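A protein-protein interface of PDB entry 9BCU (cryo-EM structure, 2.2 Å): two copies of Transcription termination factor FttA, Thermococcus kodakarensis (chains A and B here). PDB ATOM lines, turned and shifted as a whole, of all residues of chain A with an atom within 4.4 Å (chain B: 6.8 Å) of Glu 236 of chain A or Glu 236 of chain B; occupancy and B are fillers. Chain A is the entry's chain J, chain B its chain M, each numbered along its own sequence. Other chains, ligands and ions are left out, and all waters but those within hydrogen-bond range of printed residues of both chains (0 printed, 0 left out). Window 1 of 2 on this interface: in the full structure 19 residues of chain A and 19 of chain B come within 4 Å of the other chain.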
ATOM      1  N   ARG A 187      19.613  -9.181  13.756  1.00  0.00           N
ATOM      2  CA  ARG A 187      18.885  -9.024  15.006  1.00  0.00           C
ATOM      3  C   ARG A 187      17.559  -9.766  14.932  1.00  0.00           C
ATOM      4  O   ARG A 187      16.874  -9.737  13.905  1.00  0.00           O
ATOM      5  CB  ARG A 187      18.637  -7.546  15.313  1.00  0.00           C
ATOM      6  CG  ARG A 187      18.753  -7.188  16.782  1.00  0.00           C
ATOM      7  CD  ARG A 187      18.836  -5.684  16.967  1.00  0.00           C
ATOM      8  NE  ARG A 187      17.526  -5.054  16.870  1.00  0.00           N
ATOM      9  CZ  ARG A 187      16.985  -4.305  17.821  1.00  0.00           C
ATOM     10  NH1 ARG A 187      17.619  -4.063  18.956  1.00  0.00           N
ATOM     11  NH2 ARG A 187      15.777  -3.783  17.626  1.00  0.00           N
ATOM     12  N   THR A 189      13.988 -10.090  17.093  1.00  0.00           N
ATOM     13  CA  THR A 189      13.141  -9.540  18.142  1.00  0.00           C
ATOM     14  C   THR A 189      11.765 -10.183  18.070  1.00  0.00           C
ATOM     15  O   THR A 189      11.206 -10.355  16.982  1.00  0.00           O
ATOM     16  CB  THR A 189      13.008  -8.016  18.021  1.00  0.00           C
ATOM     17  OG1 THR A 189      14.295  -7.440  17.767  1.00  0.00           O
ATOM     18  CG2 THR A 189      12.436  -7.422  19.298  1.00  0.00           C
ATOM     19  N   GLN A 205      15.679  -8.495  11.695  1.00  0.00           N
ATOM     20  CA  GLN A 205      16.208  -7.184  11.349  1.00  0.00           C
ATOM     21  C   GLN A 205      17.672  -7.295  10.956  1.00  0.00           C
ATOM     22  O   GLN A 205      18.467  -7.919  11.665  1.00  0.00           O
ATOM     23  CB  GLN A 205      16.057  -6.202  12.513  1.00  0.00           C
ATOM     24  CG  GLN A 205      14.641  -6.066  13.032  1.00  0.00           C
ATOM     25  CD  GLN A 205      14.586  -5.976  14.540  1.00  0.00           C
ATOM     26  OE1 GLN A 205      15.492  -5.438  15.176  1.00  0.00           O
ATOM     27  NE2 GLN A 205      13.519  -6.504  15.123  1.00  0.00           N
ATOM     28  N   ALA A 234       6.439  -1.619  19.988  1.00  0.00           N
ATOM     29  CA  ALA A 234       7.880  -1.815  19.902  1.00  0.00           C
ATOM     30  C   ALA A 234       8.498  -0.728  19.030  1.00  0.00           C
ATOM     31  O   ALA A 234       8.005  -0.477  17.924  1.00  0.00           O
ATOM     32  CB  ALA A 234       8.201  -3.195  19.334  1.00  0.00           C
ATOM     33  N   PRO A 235       9.549  -0.046  19.499  1.00  0.00           N
ATOM     34  CA  PRO A 235      10.151   1.022  18.680  1.00  0.00           C
ATOM     35  C   PRO A 235      10.671   0.543  17.335  1.00  0.00           C
ATOM     36  O   PRO A 235      10.551   1.267  16.339  1.00  0.00           O
ATOM     37  CB  PRO A 235      11.284   1.548  19.575  1.00  0.00           C
ATOM     38  CG  PRO A 235      10.900   1.142  20.962  1.00  0.00           C
ATOM     39  CD  PRO A 235      10.189  -0.165  20.818  1.00  0.00           C
ATOM     40  N   GLU A 236      11.242  -0.663  17.277  1.00  0.00           N
ATOM     41  CA  GLU A 236      11.719  -1.189  16.002  1.00  0.00           C
ATOM     42  C   GLU A 236      10.564  -1.458  15.046  1.00  0.00           C
ATOM     43  O   GLU A 236      10.639  -1.115  13.860  1.00  0.00           O
ATOM     44  CB  GLU A 236      12.537  -2.461  16.231  1.00  0.00           C
ATOM     45  CG  GLU A 236      11.978  -3.381  17.305  1.00  0.00           C
ATOM     46  CD  GLU A 236      12.677  -3.214  18.639  1.00  0.00           C
ATOM     47  OE1 GLU A 236      12.518  -2.145  19.265  1.00  0.00           O
ATOM     48  OE2 GLU A 236      13.386  -4.152  19.060  1.00  0.00           O
ATOM     49  N   PHE A 237       9.481  -2.059  15.547  1.00  0.00           N
ATOM     50  CA  PHE A 237       8.319  -2.317  14.703  1.00  0.00           C
ATOM     51  C   PHE A 237       7.657  -1.019  14.263  1.00  0.00           C
ATOM     52  O   PHE A 237       7.206  -0.905  13.117  1.00  0.00           O
ATOM     53  CB  PHE A 237       7.320  -3.207  15.442  1.00  0.00           C
ATOM     54  CG  PHE A 237       6.345  -3.902  14.537  1.00  0.00           C
ATOM     55  CD1 PHE A 237       6.738  -4.349  13.287  1.00  0.00           C
ATOM     56  CD2 PHE A 237       5.035  -4.107  14.936  1.00  0.00           C
ATOM     57  CE1 PHE A 237       5.843  -4.988  12.450  1.00  0.00           C
ATOM     58  CE2 PHE A 237       4.135  -4.746  14.105  1.00  0.00           C
ATOM     59  CZ  PHE A 237       4.540  -5.187  12.861  1.00  0.00           C
ATOM     60  N   ARG A 238       7.584  -0.032  15.160  1.00  0.00           N
ATOM     61  CA  ARG A 238       7.021   1.264  14.794  1.00  0.00           C
ATOM     62  C   ARG A 238       7.861   1.949  13.724  1.00  0.00           C
ATOM     63  O   ARG A 238       7.319   2.540  12.783  1.00  0.00           O
ATOM     64  CB  ARG A 238       6.900   2.152  16.032  1.00  0.00           C
ATOM     65  CG  ARG A 238       5.754   1.776  16.954  1.00  0.00           C
ATOM     66  CD  ARG A 238       5.172   2.998  17.643  1.00  0.00           C
ATOM     67  NE  ARG A 238       3.916   2.695  18.317  1.00  0.00           N
ATOM     68  CZ  ARG A 238       3.585   3.143  19.520  1.00  0.00           C
ATOM     69  NH1 ARG A 238       4.395   3.924  20.214  1.00  0.00           N
ATOM     70  NH2 ARG A 238       2.409   2.799  20.039  1.00  0.00           N
ATOM     71  N   TYR A 239       9.189   1.880  13.852  1.00  0.00           N
ATOM     72  CA  TYR A 239      10.066   2.466  12.845  1.00  0.00           C
ATOM     73  C   TYR A 239       9.929   1.751  11.506  1.00  0.00           C
ATOM     74  O   TYR A 239       9.950   2.393  10.449  1.00  0.00           O
ATOM     75  CB  TYR A 239      11.515   2.429  13.327  1.00  0.00           C
ATOM     76  CG  TYR A 239      12.527   2.824  12.275  1.00  0.00           C
ATOM     77  CD1 TYR A 239      12.649   4.144  11.863  1.00  0.00           C
ATOM     78  CD2 TYR A 239      13.360   1.876  11.695  1.00  0.00           C
ATOM     79  CE1 TYR A 239      13.573   4.510  10.902  1.00  0.00           C
ATOM     80  CE2 TYR A 239      14.286   2.232  10.734  1.00  0.00           C
ATOM     81  CZ  TYR A 239      14.387   3.550  10.341  1.00  0.00           C
ATOM     82  OH  TYR A 239      15.309   3.909   9.384  1.00  0.00           O
ATOM     83  N   VAL A 240       9.798   0.423  11.531  1.00  0.00           N
ATOM     84  CA  VAL A 240       9.653  -0.335  10.292  1.00  0.00           C
ATOM     85  C   VAL A 240       8.328  -0.007   9.611  1.00  0.00           C
ATOM     86  O   VAL A 240       8.280   0.221   8.395  1.00  0.00           O
ATOM     87  CB  VAL A 240       9.793  -1.842  10.577  1.00  0.00           C
ATOM     88  CG1 VAL A 240       9.197  -2.666   9.448  1.00  0.00           C
ATOM     89  CG2 VAL A 240      11.255  -2.204  10.789  1.00  0.00           C
ATOM     90  N   ARG B 187      12.825  -2.005  28.827  1.00  0.00           N
ATOM     91  CA  ARG B 187      13.893  -2.686  28.112  1.00  0.00           C
ATOM     92  C   ARG B 187      15.069  -1.736  27.946  1.00  0.00           C
ATOM     93  O   ARG B 187      14.903  -0.513  27.935  1.00  0.00           O
ATOM     94  CB  ARG B 187      13.420  -3.208  26.746  1.00  0.00           C
ATOM     95  CG  ARG B 187      13.382  -2.163  25.645  1.00  0.00           C
ATOM     96  CD  ARG B 187      12.347  -2.510  24.591  1.00  0.00           C
ATOM     97  NE  ARG B 187      12.820  -3.543  23.678  1.00  0.00           N
ATOM     98  CZ  ARG B 187      13.034  -3.356  22.383  1.00  0.00           C
ATOM     99  NH1 ARG B 187      12.836  -2.180  21.812  1.00  0.00           N
ATOM    100  NH2 ARG B 187      13.458  -4.376  21.642  1.00  0.00           N
ATOM    101  N   ILE B 188      16.264  -2.310  27.838  1.00  0.00           N
ATOM    102  CA  ILE B 188      17.494  -1.550  27.658  1.00  0.00           C
ATOM    103  C   ILE B 188      18.232  -2.106  26.450  1.00  0.00           C
ATOM    104  O   ILE B 188      18.476  -3.315  26.369  1.00  0.00           O
ATOM    105  CB  ILE B 188      18.391  -1.599  28.910  1.00  0.00           C
ATOM    106  CG1 ILE B 188      18.304  -2.972  29.579  1.00  0.00           C
ATOM    107  CG2 ILE B 188      18.000  -0.504  29.888  1.00  0.00           C
ATOM    108  CD1 ILE B 188      19.245  -3.138  30.752  1.00  0.00           C
ATOM    109  N   THR B 189      18.587  -1.229  25.517  1.00  0.00           N
ATOM    110  CA  THR B 189      19.321  -1.603  24.316  1.00  0.00           C
ATOM    111  C   THR B 189      20.697  -0.955  24.347  1.00  0.00           C
ATOM    112  O   THR B 189      20.812   0.257  24.556  1.00  0.00           O
ATOM    113  CB  THR B 189      18.568  -1.181  23.052  1.00  0.00           C
ATOM    114  OG1 THR B 189      17.210  -1.631  23.129  1.00  0.00           O
ATOM    115  CG2 THR B 189      19.226  -1.777  21.817  1.00  0.00           C
ATOM    116  N   LEU B 191      23.506   0.410  22.410  1.00  0.00           N
ATOM    117  CA  LEU B 191      23.984   0.878  21.116  1.00  0.00           C
ATOM    118  C   LEU B 191      25.502   0.938  21.044  1.00  0.00           C
ATOM    119  O   LEU B 191      26.055   1.013  19.941  1.00  0.00           O
ATOM    120  CB  LEU B 191      23.395   2.255  20.803  1.00  0.00           C
ATOM    121  CG  LEU B 191      21.976   2.508  21.313  1.00  0.00           C
ATOM    122  CD1 LEU B 191      21.697   3.999  21.407  1.00  0.00           C
ATOM    123  CD2 LEU B 191      20.957   1.823  20.417  1.00  0.00           C
ATOM    124  N   LEU B 203      20.595   2.885  26.064  1.00  0.00           N
ATOM    125  CA  LEU B 203      19.282   3.467  25.819  1.00  0.00           C
ATOM    126  C   LEU B 203      18.250   2.732  26.661  1.00  0.00           C
ATOM    127  O   LEU B 203      18.009   1.539  26.451  1.00  0.00           O
ATOM    128  CB  LEU B 203      18.916   3.393  24.335  1.00  0.00           C
ATOM    129  CG  LEU B 203      17.564   3.985  23.935  1.00  0.00           C
ATOM    130  CD1 LEU B 203      17.583   5.500  24.049  1.00  0.00           C
ATOM    131  CD2 LEU B 203      17.183   3.555  22.527  1.00  0.00           C
ATOM    132  N   GLN B 205      14.466   2.268  27.458  1.00  0.00           N
ATOM    133  CA  GLN B 205      13.207   2.471  26.756  1.00  0.00           C
ATOM    134  C   GLN B 205      12.056   1.929  27.589  1.00  0.00           C
ATOM    135  O   GLN B 205      12.104   0.787  28.057  1.00  0.00           O
ATOM    136  CB  GLN B 205      13.223   1.793  25.384  1.00  0.00           C
ATOM    137  CG  GLN B 205      14.559   1.861  24.670  1.00  0.00           C
ATOM    138  CD  GLN B 205      14.845   0.617  23.857  1.00  0.00           C
ATOM    139  OE1 GLN B 205      15.660  -0.218  24.244  1.00  0.00           O
ATOM    140  NE2 GLN B 205      14.171   0.486  22.720  1.00  0.00           N
ATOM    141  N   TYR B 210      11.844   7.615  26.781  1.00  0.00           N
ATOM    142  CA  TYR B 210      13.108   7.035  26.344  1.00  0.00           C
ATOM    143  C   TYR B 210      14.251   7.845  26.935  1.00  0.00           C
ATOM    144  O   TYR B 210      14.242   9.079  26.868  1.00  0.00           O
ATOM    145  CB  TYR B 210      13.207   7.012  24.816  1.00  0.00           C
ATOM    146  CG  TYR B 210      12.076   6.275  24.138  1.00  0.00           C
ATOM    147  CD1 TYR B 210      12.138   4.903  23.939  1.00  0.00           C
ATOM    148  CD2 TYR B 210      10.947   6.951  23.696  1.00  0.00           C
ATOM    149  CE1 TYR B 210      11.107   4.223  23.319  1.00  0.00           C
ATOM    150  CE2 TYR B 210       9.911   6.280  23.076  1.00  0.00           C
ATOM    151  CZ  TYR B 210       9.997   4.916  22.890  1.00  0.00           C
ATOM    152  OH  TYR B 210       8.967   4.243  22.273  1.00  0.00           O
ATOM    153  N   ASP B 233      22.312   3.090  13.518  1.00  0.00           N
ATOM    154  CA  ASP B 233      21.456   2.317  12.631  1.00  0.00           C
ATOM    155  C   ASP B 233      20.461   1.439  13.377  1.00  0.00           C
ATOM    156  O   ASP B 233      19.705   0.703  12.733  1.00  0.00           O
ATOM    157  CB  ASP B 233      22.309   1.450  11.700  1.00  0.00           C
ATOM    158  CG  ASP B 233      23.504   0.840  12.405  1.00  0.00           C
ATOM    159  OD1 ASP B 233      23.636   1.034  13.631  1.00  0.00           O
ATOM    160  OD2 ASP B 233      24.314   0.168  11.732  1.00  0.00           O
ATOM    161  N   ALA B 234      20.452   1.485  14.704  1.00  0.00           N
ATOM    162  CA  ALA B 234      19.483   0.714  15.472  1.00  0.00           C
ATOM    163  C   ALA B 234      18.076   1.234  15.197  1.00  0.00           C
ATOM    164  O   ALA B 234      17.852   2.450  15.240  1.00  0.00           O
ATOM    165  CB  ALA B 234      19.794   0.796  16.963  1.00  0.00           C
ATOM    166  N   PRO B 235      17.115   0.357  14.886  1.00  0.00           N
ATOM    167  CA  PRO B 235      15.751   0.838  14.598  1.00  0.00           C
ATOM    168  C   PRO B 235      15.111   1.599  15.746  1.00  0.00           C
ATOM    169  O   PRO B 235      14.398   2.581  15.507  1.00  0.00           O
ATOM    170  CB  PRO B 235      14.989  -0.456  14.276  1.00  0.00           C
ATOM    171  CG  PRO B 235      16.043  -1.430  13.864  1.00  0.00           C
ATOM    172  CD  PRO B 235      17.247  -1.096  14.687  1.00  0.00           C
ATOM    173  N   GLU B 236      15.351   1.180  16.991  1.00  0.00           N
ATOM    174  CA  GLU B 236      14.795   1.906  18.129  1.00  0.00           C
ATOM    175  C   GLU B 236      15.415   3.291  18.258  1.00  0.00           C
ATOM    176  O   GLU B 236      14.706   4.275  18.497  1.00  0.00           O
ATOM    177  CB  GLU B 236      14.992   1.103  19.418  1.00  0.00           C
ATOM    178  CG  GLU B 236      16.358   0.456  19.555  1.00  0.00           C
ATOM    179  CD  GLU B 236      16.361  -0.994  19.120  1.00  0.00           C
ATOM    180  OE1 GLU B 236      16.490  -1.249  17.906  1.00  0.00           O
ATOM    181  OE2 GLU B 236      16.234  -1.878  19.993  1.00  0.00           O
ATOM    182  N   PHE B 237      16.737   3.390  18.095  1.00  0.00           N
ATOM    183  CA  PHE B 237      17.396   4.690  18.156  1.00  0.00           C
ATOM    184  C   PHE B 237      16.962   5.585  17.002  1.00  0.00           C
ATOM    185  O   PHE B 237      16.776   6.794  17.184  1.00  0.00           O
ATOM    186  CB  PHE B 237      18.914   4.513  18.157  1.00  0.00           C
ATOM    187  CG  PHE B 237      19.657   5.669  18.761  1.00  0.00           C
ATOM    188  CD1 PHE B 237      19.100   6.401  19.796  1.00  0.00           C
ATOM    189  CD2 PHE B 237      20.911   6.025  18.292  1.00  0.00           C
ATOM    190  CE1 PHE B 237      19.780   7.467  20.354  1.00  0.00           C
ATOM    191  CE2 PHE B 237      21.596   7.091  18.847  1.00  0.00           C
ATOM    192  CZ  PHE B 237      21.029   7.812  19.878  1.00  0.00           C
ATOM    193  N   ARG B 238      16.800   5.009  15.807  1.00  0.00           N
ATOM    194  CA  ARG B 238      16.318   5.783  14.668  1.00  0.00           C
ATOM    195  C   ARG B 238      14.906   6.303  14.912  1.00  0.00           C
ATOM    196  O   ARG B 238      14.600   7.459  14.600  1.00  0.00           O
ATOM    197  CB  ARG B 238      16.362   4.935  13.398  1.00  0.00           C
ATOM    198  CG  ARG B 238      17.757   4.715  12.844  1.00  0.00           C
ATOM    199  CD  ARG B 238      18.010   5.576  11.619  1.00  0.00           C
ATOM    200  NE  ARG B 238      17.781   4.841  10.382  1.00  0.00           N
ATOM    201  CZ  ARG B 238      18.744   4.347   9.615  1.00  0.00           C
ATOM    202  NH1 ARG B 238      20.021   4.493   9.929  1.00  0.00           N
ATOM    203  NH2 ARG B 238      18.418   3.691   8.505  1.00  0.00           N
ATOM    204  N   TYR B 239      14.035   5.461  15.472  1.00  0.00           N
ATOM    205  CA  TYR B 239      12.674   5.890  15.780  1.00  0.00           C
ATOM    206  C   TYR B 239      12.663   6.979  16.847  1.00  0.00           C
ATOM    207  O   TYR B 239      11.870   7.923  16.768  1.00  0.00           O
ATOM    208  CB  TYR B 239      11.838   4.692  16.225  1.00  0.00           C
ATOM    209  CG  TYR B 239      10.466   5.053  16.746  1.00  0.00           C
ATOM    210  CD1 TYR B 239       9.479   5.523  15.889  1.00  0.00           C
ATOM    211  CD2 TYR B 239      10.157   4.922  18.093  1.00  0.00           C
ATOM    212  CE1 TYR B 239       8.223   5.853  16.361  1.00  0.00           C
ATOM    213  CE2 TYR B 239       8.904   5.250  18.574  1.00  0.00           C
ATOM    214  CZ  TYR B 239       7.941   5.715  17.704  1.00  0.00           C
ATOM    215  OH  TYR B 239       6.693   6.042  18.179  1.00  0.00           O
ATOM    216  N   VAL B 240      13.529   6.856  17.855  1.00  0.00           N
ATOM    217  CA  VAL B 240      13.581   7.852  18.922  1.00  0.00           C
ATOM    218  C   VAL B 240      14.085   9.188  18.386  1.00  0.00           C
ATOM    219  O   VAL B 240      13.517  10.247  18.679  1.00  0.00           O
ATOM    220  CB  VAL B 240      14.450   7.339  20.085  1.00  0.00           C
ATOM    221  CG1 VAL B 240      14.895   8.488  20.976  1.00  0.00           C
ATOM    222  CG2 VAL B 240      13.690   6.300  20.893  1.00  0.00           C
ATOM    223  N   LEU B 241      15.149   9.160  17.580  1.00  0.00           N
ATOM    224  CA  LEU B 241      15.753  10.403  17.108  1.00  0.00           C
ATOM    225  C   LEU B 241      14.898  11.075  16.040  1.00  0.00           C
ATOM    226  O   LEU B 241      14.782  12.306  16.019  1.00  0.00           O
ATOM    227  CB  LEU B 241      17.160  10.132  16.577  1.00  0.00           C
ATOM    228  CG  LEU B 241      18.269   9.983  17.620  1.00  0.00           C
ATOM    229  CD1 LEU B 241      19.634   9.981  16.952  1.00  0.00           C
ATOM    230  CD2 LEU B 241      18.182  11.087  18.663  1.00  0.00           C
ATOM    231  N   LEU B 642      23.577  -3.957  20.283  1.00  0.00           N
ATOM    232  CA  LEU B 642      22.249  -4.071  19.671  1.00  0.00           C
ATOM    233  C   LEU B 642      21.442  -5.210  20.291  1.00  0.00           C
ATOM    234  O   LEU B 642      20.726  -5.936  19.601  1.00  0.00           O
ATOM    235  CB  LEU B 642      22.348  -4.239  18.152  1.00  0.00           C
ATOM    236  CG  LEU B 642      23.028  -3.099  17.395  1.00  0.00           C
ATOM    237  CD1 LEU B 642      23.007  -3.362  15.900  1.00  0.00           C
ATOM    238  CD2 LEU B 642      22.354  -1.780  17.720  1.00  0.00           C
ATOM    239  N   ASP B 643      21.558  -5.368  21.606  1.00  0.00           N
ATOM    240  CA  ASP B 643      20.828  -6.386  22.348  1.00  0.00           C
ATOM    241  C   ASP B 643      19.883  -5.705  23.325  1.00  0.00           C
ATOM    242  O   ASP B 643      20.312  -4.880  24.138  1.00  0.00           O
ATOM    243  CB  ASP B 643      21.785  -7.318  23.096  1.00  0.00           C
ATOM    244  CG  ASP B 643      21.865  -8.696  22.470  1.00  0.00           C
ATOM    245  OD1 ASP B 643      21.422  -8.850  21.312  1.00  0.00           O
ATOM    246  OD2 ASP B 643      22.370  -9.624  23.135  1.00  0.00           O
ATOM    247  N   ALA B 644      18.602  -6.051  23.244  1.00  0.00           N
ATOM    248  CA  ALA B 644      17.580  -5.500  24.121  1.00  0.00           C
ATOM    249  C   ALA B 644      17.176  -6.549  25.146  1.00  0.00           C
ATOM    250  O   ALA B 644      16.823  -7.676  24.782  1.00  0.00           O
ATOM    251  CB  ALA B 644      16.358  -5.037  23.324  1.00  0.00           C
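The guanidinium group of Arg 187 of chain A is in salt-bridge range of the side-chain carboxylate of Glu 236 of chain B.
OE1 of Glu 236 of chain A is in salt-bridge range of NH1 of Arg 187 of chain B (2.6 Å).
OH of Tyr 239 of chain A is in hydrogen-bond range of NE of Arg 238 of chain B (2.8 Å).
OE1 of Gln 205 of chain A sits at hydrogen-bond distance from NE of Arg 187 of chain A, 2.7 Å away.
OE2 of Glu 236 of chain A is in salt-bridge range of NH2 of Arg 187 of chain A.
The side-chain hydroxyl (OG1) of Thr 189 of chain A sits at hydrogen-bond distance from the side-chain amide nitrogen (NE2) of Gln 205 of chain A (2.9 Å).
O of Arg 187 of chain B lies within hydrogen-bond range of N of Gln 205 of chain B (2.9 Å).
N of Thr 189 of chain B sits at hydrogen-bond distance from O of Leu 203 of chain B (3.0 Å).
The backbone NH (N) of Thr 189 of chain B sits close to the side-chain amide oxygen (OE1) of Gln 205 of chain B, 3.3 Å away.
Arg 187 of chain A touches Glu 236 of chain B, and with the chains exchanged Glu 236 of chain A touches Arg 187 of chain B.
Pro 235 of chain A touches Arg 187 of chain B, but with the chains exchanged Arg 187 of chain A does not touch Pro 235 of chain B (4.2 Å).
Pro 235 of chain A touches Gln 205 of chain B, but with the chains exchanged Gln 205 of chain A does not touch Pro 235 of chain B (4.3 Å).
Arg 238 of chain A touches Tyr 239 of chain B, and with the chains exchanged Tyr 239 of chain A touches Arg 238 of chain B.
10 positions are printed for both chains.
Ala 234 of chain A touches none of the printed residues of chain B.
Glu 236 of chain A touches three residues of chain B.
Of the printed residues of chain B, Tyr 239 of chain A touches Pro 235 (3.6 Å), Arg 238 (2.8 Å) and Tyr 239 (3.7 Å).
Of the printed residues of chain A, Arg 187 of chain B touches Thr 189, Pro 235 and Glu 236.
Of the printed residues of chain A, Gln 205 of chain B touches Pro 235.
Printed residues of chain A within 4 Å of Tyr 210 of chain B: Pro 235 (3.9 Å).
The nearest residue of chain B that does not touch Glu 236 of chain A is Gln 205 of chain B (4.6 Å).
Among the printed residues, merely in contact across the chains: Arg 187 of chain A with Leu 642 of chain B, Arg 238 of chain A with Tyr 239 of chain B, Pro 235 of chain A with Arg 187 of chain B, Tyr 239 of chain A with Pro 235 of chain B, Pro 235 of chain A with Tyr 239 of chain B, Tyr 239 of chain A with Tyr 239 of chain B, Glu 236 of chain A with Pro 235 of chain B, Pro 235 of chain A with Glu 236 of chain B, Glu 236 of chain A with Glu 236 of chain B, Pro 235 of chain A with Gln 205 of chain B, Pro 235 of chain A with Tyr 210 of chain B, Thr 189 of chain A with Arg 187 of chain B and Arg 187 of chain A with Thr 189 of chain B.
Of the 19 printed residues of chain B, 9 touch a printed residue of chain A.
Printed residues of chain B that touch a printed residue of chain A: Arg 187, Thr 189, Gln 205, Tyr 210, Pro 235, Glu 236, Arg 238, Tyr 239 and Leu 642.
Hydrophobic or aromatic side chains of chain B that line the printed part of chain A: Tyr 210, Pro 235, Tyr 239 and Leu 642.
Along chain A the printed residues that touch a printed residue of chain B span positions 187 to 239.
Among the printed residues, 16 pairs touch across the chains.
Among the printed residues, Asp or Glu carboxylates within 4 Å of a Lys or Arg side-chain nitrogen of the other chain: Arg 187 of chain A with Glu 236 of chain B (2.6 Å) and Glu 236 of chain A with Arg 187 of chain B (2.6 Å).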
